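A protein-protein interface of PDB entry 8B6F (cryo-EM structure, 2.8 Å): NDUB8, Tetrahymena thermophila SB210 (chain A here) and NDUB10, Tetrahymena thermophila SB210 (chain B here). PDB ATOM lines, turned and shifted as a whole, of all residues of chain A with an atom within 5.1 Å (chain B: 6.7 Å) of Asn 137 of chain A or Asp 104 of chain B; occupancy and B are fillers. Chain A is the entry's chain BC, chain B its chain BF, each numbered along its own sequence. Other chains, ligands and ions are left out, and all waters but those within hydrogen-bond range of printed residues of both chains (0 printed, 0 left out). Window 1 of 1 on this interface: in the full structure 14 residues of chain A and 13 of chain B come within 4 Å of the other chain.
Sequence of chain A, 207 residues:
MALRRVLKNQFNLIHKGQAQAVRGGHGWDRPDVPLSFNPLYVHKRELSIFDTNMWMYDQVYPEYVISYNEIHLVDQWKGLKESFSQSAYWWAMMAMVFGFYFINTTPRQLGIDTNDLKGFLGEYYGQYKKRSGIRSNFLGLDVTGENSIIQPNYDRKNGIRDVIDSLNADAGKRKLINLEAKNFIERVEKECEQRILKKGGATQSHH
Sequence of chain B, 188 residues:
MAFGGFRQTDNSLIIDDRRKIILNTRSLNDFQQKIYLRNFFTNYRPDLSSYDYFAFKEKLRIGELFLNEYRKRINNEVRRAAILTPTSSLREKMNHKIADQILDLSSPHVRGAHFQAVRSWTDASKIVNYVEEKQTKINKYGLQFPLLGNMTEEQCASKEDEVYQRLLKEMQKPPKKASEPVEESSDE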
ATOM      1  N   ARG A 135      23.719  15.344 -16.412  1.00  0.00           N
ATOM      2  CA  ARG A 135      23.146  15.866 -17.640  1.00  0.00           C
ATOM      3  C   ARG A 135      21.695  16.279 -17.412  1.00  0.00           C
ATOM      4  O   ARG A 135      21.037  15.845 -16.461  1.00  0.00           O
ATOM      5  CB  ARG A 135      23.232  14.827 -18.759  1.00  0.00           C
ATOM      6  CG  ARG A 135      24.650  14.576 -19.245  1.00  0.00           C
ATOM      7  CD  ARG A 135      24.692  13.575 -20.386  1.00  0.00           C
ATOM      8  NE  ARG A 135      24.380  12.220 -19.946  1.00  0.00           N
ATOM      9  CZ  ARG A 135      23.170  11.677 -19.955  1.00  0.00           C
ATOM     10  NH1 ARG A 135      22.110  12.352 -20.370  1.00  0.00           N
ATOM     11  NH2 ARG A 135      23.018  10.424 -19.538  1.00  0.00           N
ATOM     12  N   SER A 136      21.200  17.136 -18.298  1.00  0.00           N
ATOM     13  CA  SER A 136      19.840  17.637 -18.177  1.00  0.00           C
ATOM     14  C   SER A 136      18.832  16.510 -18.383  1.00  0.00           C
ATOM     15  O   SER A 136      19.081  15.545 -19.111  1.00  0.00           O
ATOM     16  CB  SER A 136      19.590  18.756 -19.185  1.00  0.00           C
ATOM     17  OG  SER A 136      19.758  18.291 -20.512  1.00  0.00           O
ATOM     18  N   ASN A 137      17.681  16.645 -17.730  1.00  0.00           N
ATOM     19  CA  ASN A 137      16.647  15.624 -17.809  1.00  0.00           C
ATOM     20  C   ASN A 137      16.087  15.527 -19.224  1.00  0.00           C
ATOM     21  O   ASN A 137      16.004  16.517 -19.956  1.00  0.00           O
ATOM     22  CB  ASN A 137      15.521  15.937 -16.826  1.00  0.00           C
ATOM     23  CG  ASN A 137      14.551  14.790 -16.677  1.00  0.00           C
ATOM     24  OD1 ASN A 137      14.941  13.625 -16.688  1.00  0.00           O
ATOM     25  ND2 ASN A 137      13.275  15.114 -16.546  1.00  0.00           N
ATOM     26  N   PHE A 138      15.694  14.310 -19.606  1.00  0.00           N
ATOM     27  CA  PHE A 138      15.203  14.087 -20.963  1.00  0.00           C
ATOM     28  C   PHE A 138      13.797  14.639 -21.158  1.00  0.00           C
ATOM     29  O   PHE A 138      13.419  14.975 -22.286  1.00  0.00           O
ATOM     30  CB  PHE A 138      15.244  12.594 -21.302  1.00  0.00           C
ATOM     31  CG  PHE A 138      14.233  11.766 -20.559  1.00  0.00           C
ATOM     32  CD1 PHE A 138      14.442  11.410 -19.238  1.00  0.00           C
ATOM     33  CD2 PHE A 138      13.086  11.319 -21.195  1.00  0.00           C
ATOM     34  CE1 PHE A 138      13.518  10.638 -18.560  1.00  0.00           C
ATOM     35  CE2 PHE A 138      12.159  10.547 -20.523  1.00  0.00           C
ATOM     36  CZ  PHE A 138      12.375  10.205 -19.204  1.00  0.00           C
ATOM     37  N   LEU A 139      13.007  14.733 -20.088  1.00  0.00           N
ATOM     38  CA  LEU A 139      11.667  15.300 -20.188  1.00  0.00           C
ATOM     39  C   LEU A 139      11.660  16.819 -20.119  1.00  0.00           C
ATOM     40  O   LEU A 139      10.601  17.424 -20.325  1.00  0.00           O
ATOM     41  CB  LEU A 139      10.768  14.749 -19.078  1.00  0.00           C
ATOM     42  CG  LEU A 139      10.286  13.302 -19.200  1.00  0.00           C
ATOM     43  CD1 LEU A 139       9.396  12.953 -18.021  1.00  0.00           C
ATOM     44  CD2 LEU A 139       9.550  13.062 -20.508  1.00  0.00           C
ATOM     45  N   GLY A 140      12.796  17.449 -19.844  1.00  0.00           N
ATOM     46  CA  GLY A 140      12.839  18.885 -19.680  1.00  0.00           C
ATOM     47  C   GLY A 140      12.525  19.374 -18.286  1.00  0.00           C
ATOM     48  O   GLY A 140      12.426  20.589 -18.083  1.00  0.00           O
ATOM     49  N   LEU A 141      12.357  18.472 -17.322  1.00  0.00           N
ATOM     50  CA  LEU A 141      12.098  18.889 -15.954  1.00  0.00           C
ATOM     51  C   LEU A 141      13.301  19.636 -15.394  1.00  0.00           C
ATOM     52  O   LEU A 141      14.451  19.370 -15.751  1.00  0.00           O
ATOM     53  CB  LEU A 141      11.785  17.676 -15.074  1.00  0.00           C
ATOM     54  CG  LEU A 141      10.713  16.705 -15.577  1.00  0.00           C
ATOM     55  CD1 LEU A 141      10.438  15.628 -14.537  1.00  0.00           C
ATOM     56  CD2 LEU A 141       9.444  17.432 -15.946  1.00  0.00           C
ATOM     57  N   VAL A 143      14.571  19.310 -12.653  1.00  0.00           N
ATOM     58  CA  VAL A 143      15.390  18.442 -11.819  1.00  0.00           C
ATOM     59  C   VAL A 143      16.566  17.913 -12.630  1.00  0.00           C
ATOM     60  O   VAL A 143      16.508  17.799 -13.862  1.00  0.00           O
ATOM     61  CB  VAL A 143      14.544  17.291 -11.246  1.00  0.00           C
ATOM     62  CG1 VAL A 143      14.194  16.276 -12.329  1.00  0.00           C
ATOM     63  CG2 VAL A 143      15.271  16.618 -10.094  1.00  0.00           C
ATOM     64  N   ARG B  71      12.884   2.522 -16.559  1.00  0.00           N
ATOM     65  CA  ARG B  71      14.057   2.065 -15.825  1.00  0.00           C
ATOM     66  C   ARG B  71      14.127   0.543 -15.800  1.00  0.00           C
ATOM     67  O   ARG B  71      15.203  -0.042 -15.959  1.00  0.00           O
ATOM     68  CB  ARG B  71      14.039   2.627 -14.405  1.00  0.00           C
ATOM     69  CG  ARG B  71      15.352   2.463 -13.656  1.00  0.00           C
ATOM     70  CD  ARG B  71      16.466   3.230 -14.350  1.00  0.00           C
ATOM     71  NE  ARG B  71      17.674   3.324 -13.539  1.00  0.00           N
ATOM     72  CZ  ARG B  71      18.681   2.464 -13.580  1.00  0.00           C
ATOM     73  NH1 ARG B  71      18.659   1.410 -14.377  1.00  0.00           N
ATOM     74  NH2 ARG B  71      19.739   2.669 -12.801  1.00  0.00           N
ATOM     75  N   ALA B  99      24.252   3.275 -21.808  1.00  0.00           N
ATOM     76  CA  ALA B  99      24.801   3.806 -20.563  1.00  0.00           C
ATOM     77  C   ALA B  99      24.261   5.198 -20.267  1.00  0.00           C
ATOM     78  O   ALA B  99      23.943   5.518 -19.117  1.00  0.00           O
ATOM     79  CB  ALA B  99      26.328   3.831 -20.628  1.00  0.00           C
ATOM     80  N   ASP B 100      24.163   6.045 -21.291  1.00  0.00           N
ATOM     81  CA  ASP B 100      23.617   7.383 -21.096  1.00  0.00           C
ATOM     82  C   ASP B 100      22.178   7.324 -20.603  1.00  0.00           C
ATOM     83  O   ASP B 100      21.785   8.090 -19.715  1.00  0.00           O
ATOM     84  CB  ASP B 100      23.706   8.178 -22.397  1.00  0.00           C
ATOM     85  CG  ASP B 100      25.134   8.350 -22.875  1.00  0.00           C
ATOM     86  OD1 ASP B 100      25.730   7.356 -23.340  1.00  0.00           O
ATOM     87  OD2 ASP B 100      25.662   9.478 -22.781  1.00  0.00           O
ATOM     88  N   GLN B 101      21.376   6.418 -21.166  1.00  0.00           N
ATOM     89  CA  GLN B 101      19.996   6.269 -20.717  1.00  0.00           C
ATOM     90  C   GLN B 101      19.927   5.748 -19.288  1.00  0.00           C
ATOM     91  O   GLN B 101      19.076   6.187 -18.506  1.00  0.00           O
ATOM     92  CB  GLN B 101      19.232   5.343 -21.664  1.00  0.00           C
ATOM     93  CG  GLN B 101      18.954   5.961 -23.027  1.00  0.00           C
ATOM     94  CD  GLN B 101      18.093   5.076 -23.901  1.00  0.00           C
ATOM     95  OE1 GLN B 101      17.695   3.986 -23.498  1.00  0.00           O
ATOM     96  NE2 GLN B 101      17.794   5.548 -25.107  1.00  0.00           N
ATOM     97  N   ILE B 102      20.806   4.815 -18.925  1.00  0.00           N
ATOM     98  CA  ILE B 102      20.822   4.311 -17.554  1.00  0.00           C
ATOM     99  C   ILE B 102      21.055   5.455 -16.577  1.00  0.00           C
ATOM    100  O   ILE B 102      20.366   5.579 -15.558  1.00  0.00           O
ATOM    101  CB  ILE B 102      21.905   3.228 -17.408  1.00  0.00           C
ATOM    102  CG1 ILE B 102      21.510   1.984 -18.196  1.00  0.00           C
ATOM    103  CG2 ILE B 102      22.124   2.872 -15.942  1.00  0.00           C
ATOM    104  CD1 ILE B 102      22.647   1.023 -18.389  1.00  0.00           C
ATOM    105  N   LEU B 103      22.038   6.307 -16.870  1.00  0.00           N
ATOM    106  CA  LEU B 103      22.326   7.433 -15.989  1.00  0.00           C
ATOM    107  C   LEU B 103      21.202   8.457 -16.020  1.00  0.00           C
ATOM    108  O   LEU B 103      20.866   9.050 -14.990  1.00  0.00           O
ATOM    109  CB  LEU B 103      23.657   8.076 -16.377  1.00  0.00           C
ATOM    110  CG  LEU B 103      24.916   7.322 -15.941  1.00  0.00           C
ATOM    111  CD1 LEU B 103      26.157   7.982 -16.504  1.00  0.00           C
ATOM    112  CD2 LEU B 103      25.007   7.237 -14.425  1.00  0.00           C
ATOM    113  N   ASP B 104      20.606   8.674 -17.193  1.00  0.00           N
ATOM    114  CA  ASP B 104      19.554   9.672 -17.318  1.00  0.00           C
ATOM    115  C   ASP B 104      18.259   9.235 -16.649  1.00  0.00           C
ATOM    116  O   ASP B 104      17.403  10.082 -16.373  1.00  0.00           O
ATOM    117  CB  ASP B 104      19.301   9.974 -18.795  1.00  0.00           C
ATOM    118  CG  ASP B 104      18.172  10.959 -19.001  1.00  0.00           C
ATOM    119  OD1 ASP B 104      18.258  12.083 -18.464  1.00  0.00           O
ATOM    120  OD2 ASP B 104      17.202  10.609 -19.703  1.00  0.00           O
ATOM    121  N   LEU B 105      18.089   7.938 -16.392  1.00  0.00           N
ATOM    122  CA  LEU B 105      16.932   7.421 -15.672  1.00  0.00           C
ATOM    123  C   LEU B 105      17.238   7.182 -14.198  1.00  0.00           C
ATOM    124  O   LEU B 105      16.714   6.239 -13.600  1.00  0.00           O
ATOM    125  CB  LEU B 105      16.436   6.133 -16.327  1.00  0.00           C
ATOM    126  CG  LEU B 105      15.968   6.244 -17.778  1.00  0.00           C
ATOM    127  CD1 LEU B 105      15.665   4.870 -18.343  1.00  0.00           C
ATOM    128  CD2 LEU B 105      14.748   7.142 -17.887  1.00  0.00           C
ATOM    129  N   SER B 106      18.083   8.017 -13.600  1.00  0.00           N
ATOM    130  CA  SER B 106      18.471   7.843 -12.210  1.00  0.00           C
ATOM    131  C   SER B 106      17.339   8.279 -11.282  1.00  0.00           C
ATOM    132  O   SER B 106      16.252   8.667 -11.717  1.00  0.00           O
ATOM    133  CB  SER B 106      19.750   8.623 -11.918  1.00  0.00           C
ATOM    134  OG  SER B 106      20.822   8.156 -12.718  1.00  0.00           O
ATOM    135  N   SER B 107      17.607   8.220  -9.978  1.00  0.00           N
ATOM    136  CA  SER B 107      16.553   8.453  -8.995  1.00  0.00           C
ATOM    137  C   SER B 107      15.873   9.807  -9.146  1.00  0.00           C
ATOM    138  O   SER B 107      14.635   9.856  -9.031  1.00  0.00           O
ATOM    139  CB  SER B 107      17.118   8.292  -7.578  1.00  0.00           C
ATOM    140  OG  SER B 107      17.954   9.377  -7.222  1.00  0.00           O
ATOM    141  N   PRO B 108      16.575  10.919  -9.382  1.00  0.00           N
ATOM    142  CA  PRO B 108      15.864  12.205  -9.480  1.00  0.00           C
ATOM    143  C   PRO B 108      14.830  12.224 -10.587  1.00  0.00           C
ATOM    144  O   PRO B 108      13.803  12.902 -10.459  1.00  0.00           O
ATOM    145  CB  PRO B 108      16.990  13.217  -9.742  1.00  0.00           C
ATOM    146  CG  PRO B 108      18.254  12.511  -9.383  1.00  0.00           C
ATOM    147  CD  PRO B 108      18.007  11.072  -9.684  1.00  0.00           C
ATOM    148  N   HIS B 109      15.070  11.489 -11.671  1.00  0.00           N
ATOM    149  CA  HIS B 109      14.186  11.505 -12.826  1.00  0.00           C
ATOM    150  C   HIS B 109      13.126  10.417 -12.769  1.00  0.00           C
ATOM    151  O   HIS B 109      12.050  10.581 -13.353  1.00  0.00           O
ATOM    152  CB  HIS B 109      15.009  11.350 -14.107  1.00  0.00           C
ATOM    153  CG  HIS B 109      16.282  12.137 -14.095  1.00  0.00           C
ATOM    154  ND1 HIS B 109      16.329  13.483 -14.389  1.00  0.00           N
ATOM    155  CD2 HIS B 109      17.554  11.768 -13.819  1.00  0.00           C
ATOM    156  CE1 HIS B 109      17.576  13.908 -14.295  1.00  0.00           C
ATOM    157  NE2 HIS B 109      18.339  12.888 -13.950  1.00  0.00           N
ATOM    158  N   VAL B 110      13.402   9.311 -12.082  1.00  0.00           N
ATOM    159  CA  VAL B 110      12.437   8.234 -11.905  1.00  0.00           C
ATOM    160  C   VAL B 110      12.420   7.851 -10.432  1.00  0.00           C
ATOM    161  O   VAL B 110      13.477   7.663  -9.823  1.00  0.00           O
ATOM    162  CB  VAL B 110      12.773   7.014 -12.788  1.00  0.00           C
ATOM    163  CG1 VAL B 110      13.029   7.456 -14.218  1.00  0.00           C
ATOM    164  CG2 VAL B 110      13.970   6.239 -12.248  1.00  0.00           C
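The guanidinium group (NE) of Arg 71 of chain B sits at hydrogen-bond distance from the backbone carbonyl oxygen (O) of Leu 105 of chain B (3.1 Å).
The backbone carbonyl oxygen (O) of Leu 103 of chain B is in hydrogen-bond range of the side-chain hydroxyl (OG) of Ser 106 of chain B, at 2.4 Å.
Of the printed residues of chain B, Asn 137 of chain A touches Asp 104 (3.9 Å) and His 109 (2.7 Å).
Of chain A, only Arg 135 (3.8 Å), Ser 136 (3.6 Å), Asn 137 (3.9 Å) and Phe 138 (2.9 Å) come within 4 Å of Asp 104 of chain B.
Printed residues of chain A within 4 Å of His 109 of chain B: Asn 137.
Of the printed residues of chain B, Ser 136 of chain A touches Asp 104 (3.6 Å).
Of the printed residues of chain B, Phe 138 of chain A touches Asp 104 (2.9 Å) and Leu 105 (3.8 Å).
Of the printed residues of chain B, Arg 135 of chain A touches Asp 100 (2.6 Å), Leu 103 (3.99 Å) and Asp 104 (3.8 Å).
Gly 140 of chain A touches none of the printed residues of chain B.
The nearest residue of chain B that does not touch Asn 137 of chain A is Pro 108 of chain B (6.3 Å).
Among the printed residues, pairs that only touch across the chains: Phe 138 of chain A with Asp 104 of chain B, Ser 136 of chain A with Asp 104 of chain B, Phe 138 of chain A with Leu 105 of chain B, Arg 135 of chain A with Asp 104 of chain B, Val 143 of chain A with Pro 108 of chain B, Asn 137 of chain A with Asp 104 of chain B and Arg 135 of chain A with Leu 103 of chain B.
NH2 of Arg 135 of chain A lies within hydrogen-bond range of O of Asp 100 of chain B, 2.6 Å away.
The side-chain amide oxygen of Asn 137 of chain A sits at hydrogen-bond distance from a ring nitrogen (ND1) of His 109 of chain B (2.7 Å).
Of the 13 printed residues of chain B, 6 touch a printed residue of chain A.
Along chain B the printed residues that touch a printed residue of chain A span positions 100 to 109.
Along chain A the printed residues that touch a printed residue of chain B span positions 135 to 143.
Among the printed residues, no Asp or Glu carboxylate lies within 4 Å of a Lys or Arg side-chain nitrogen of the other chain.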
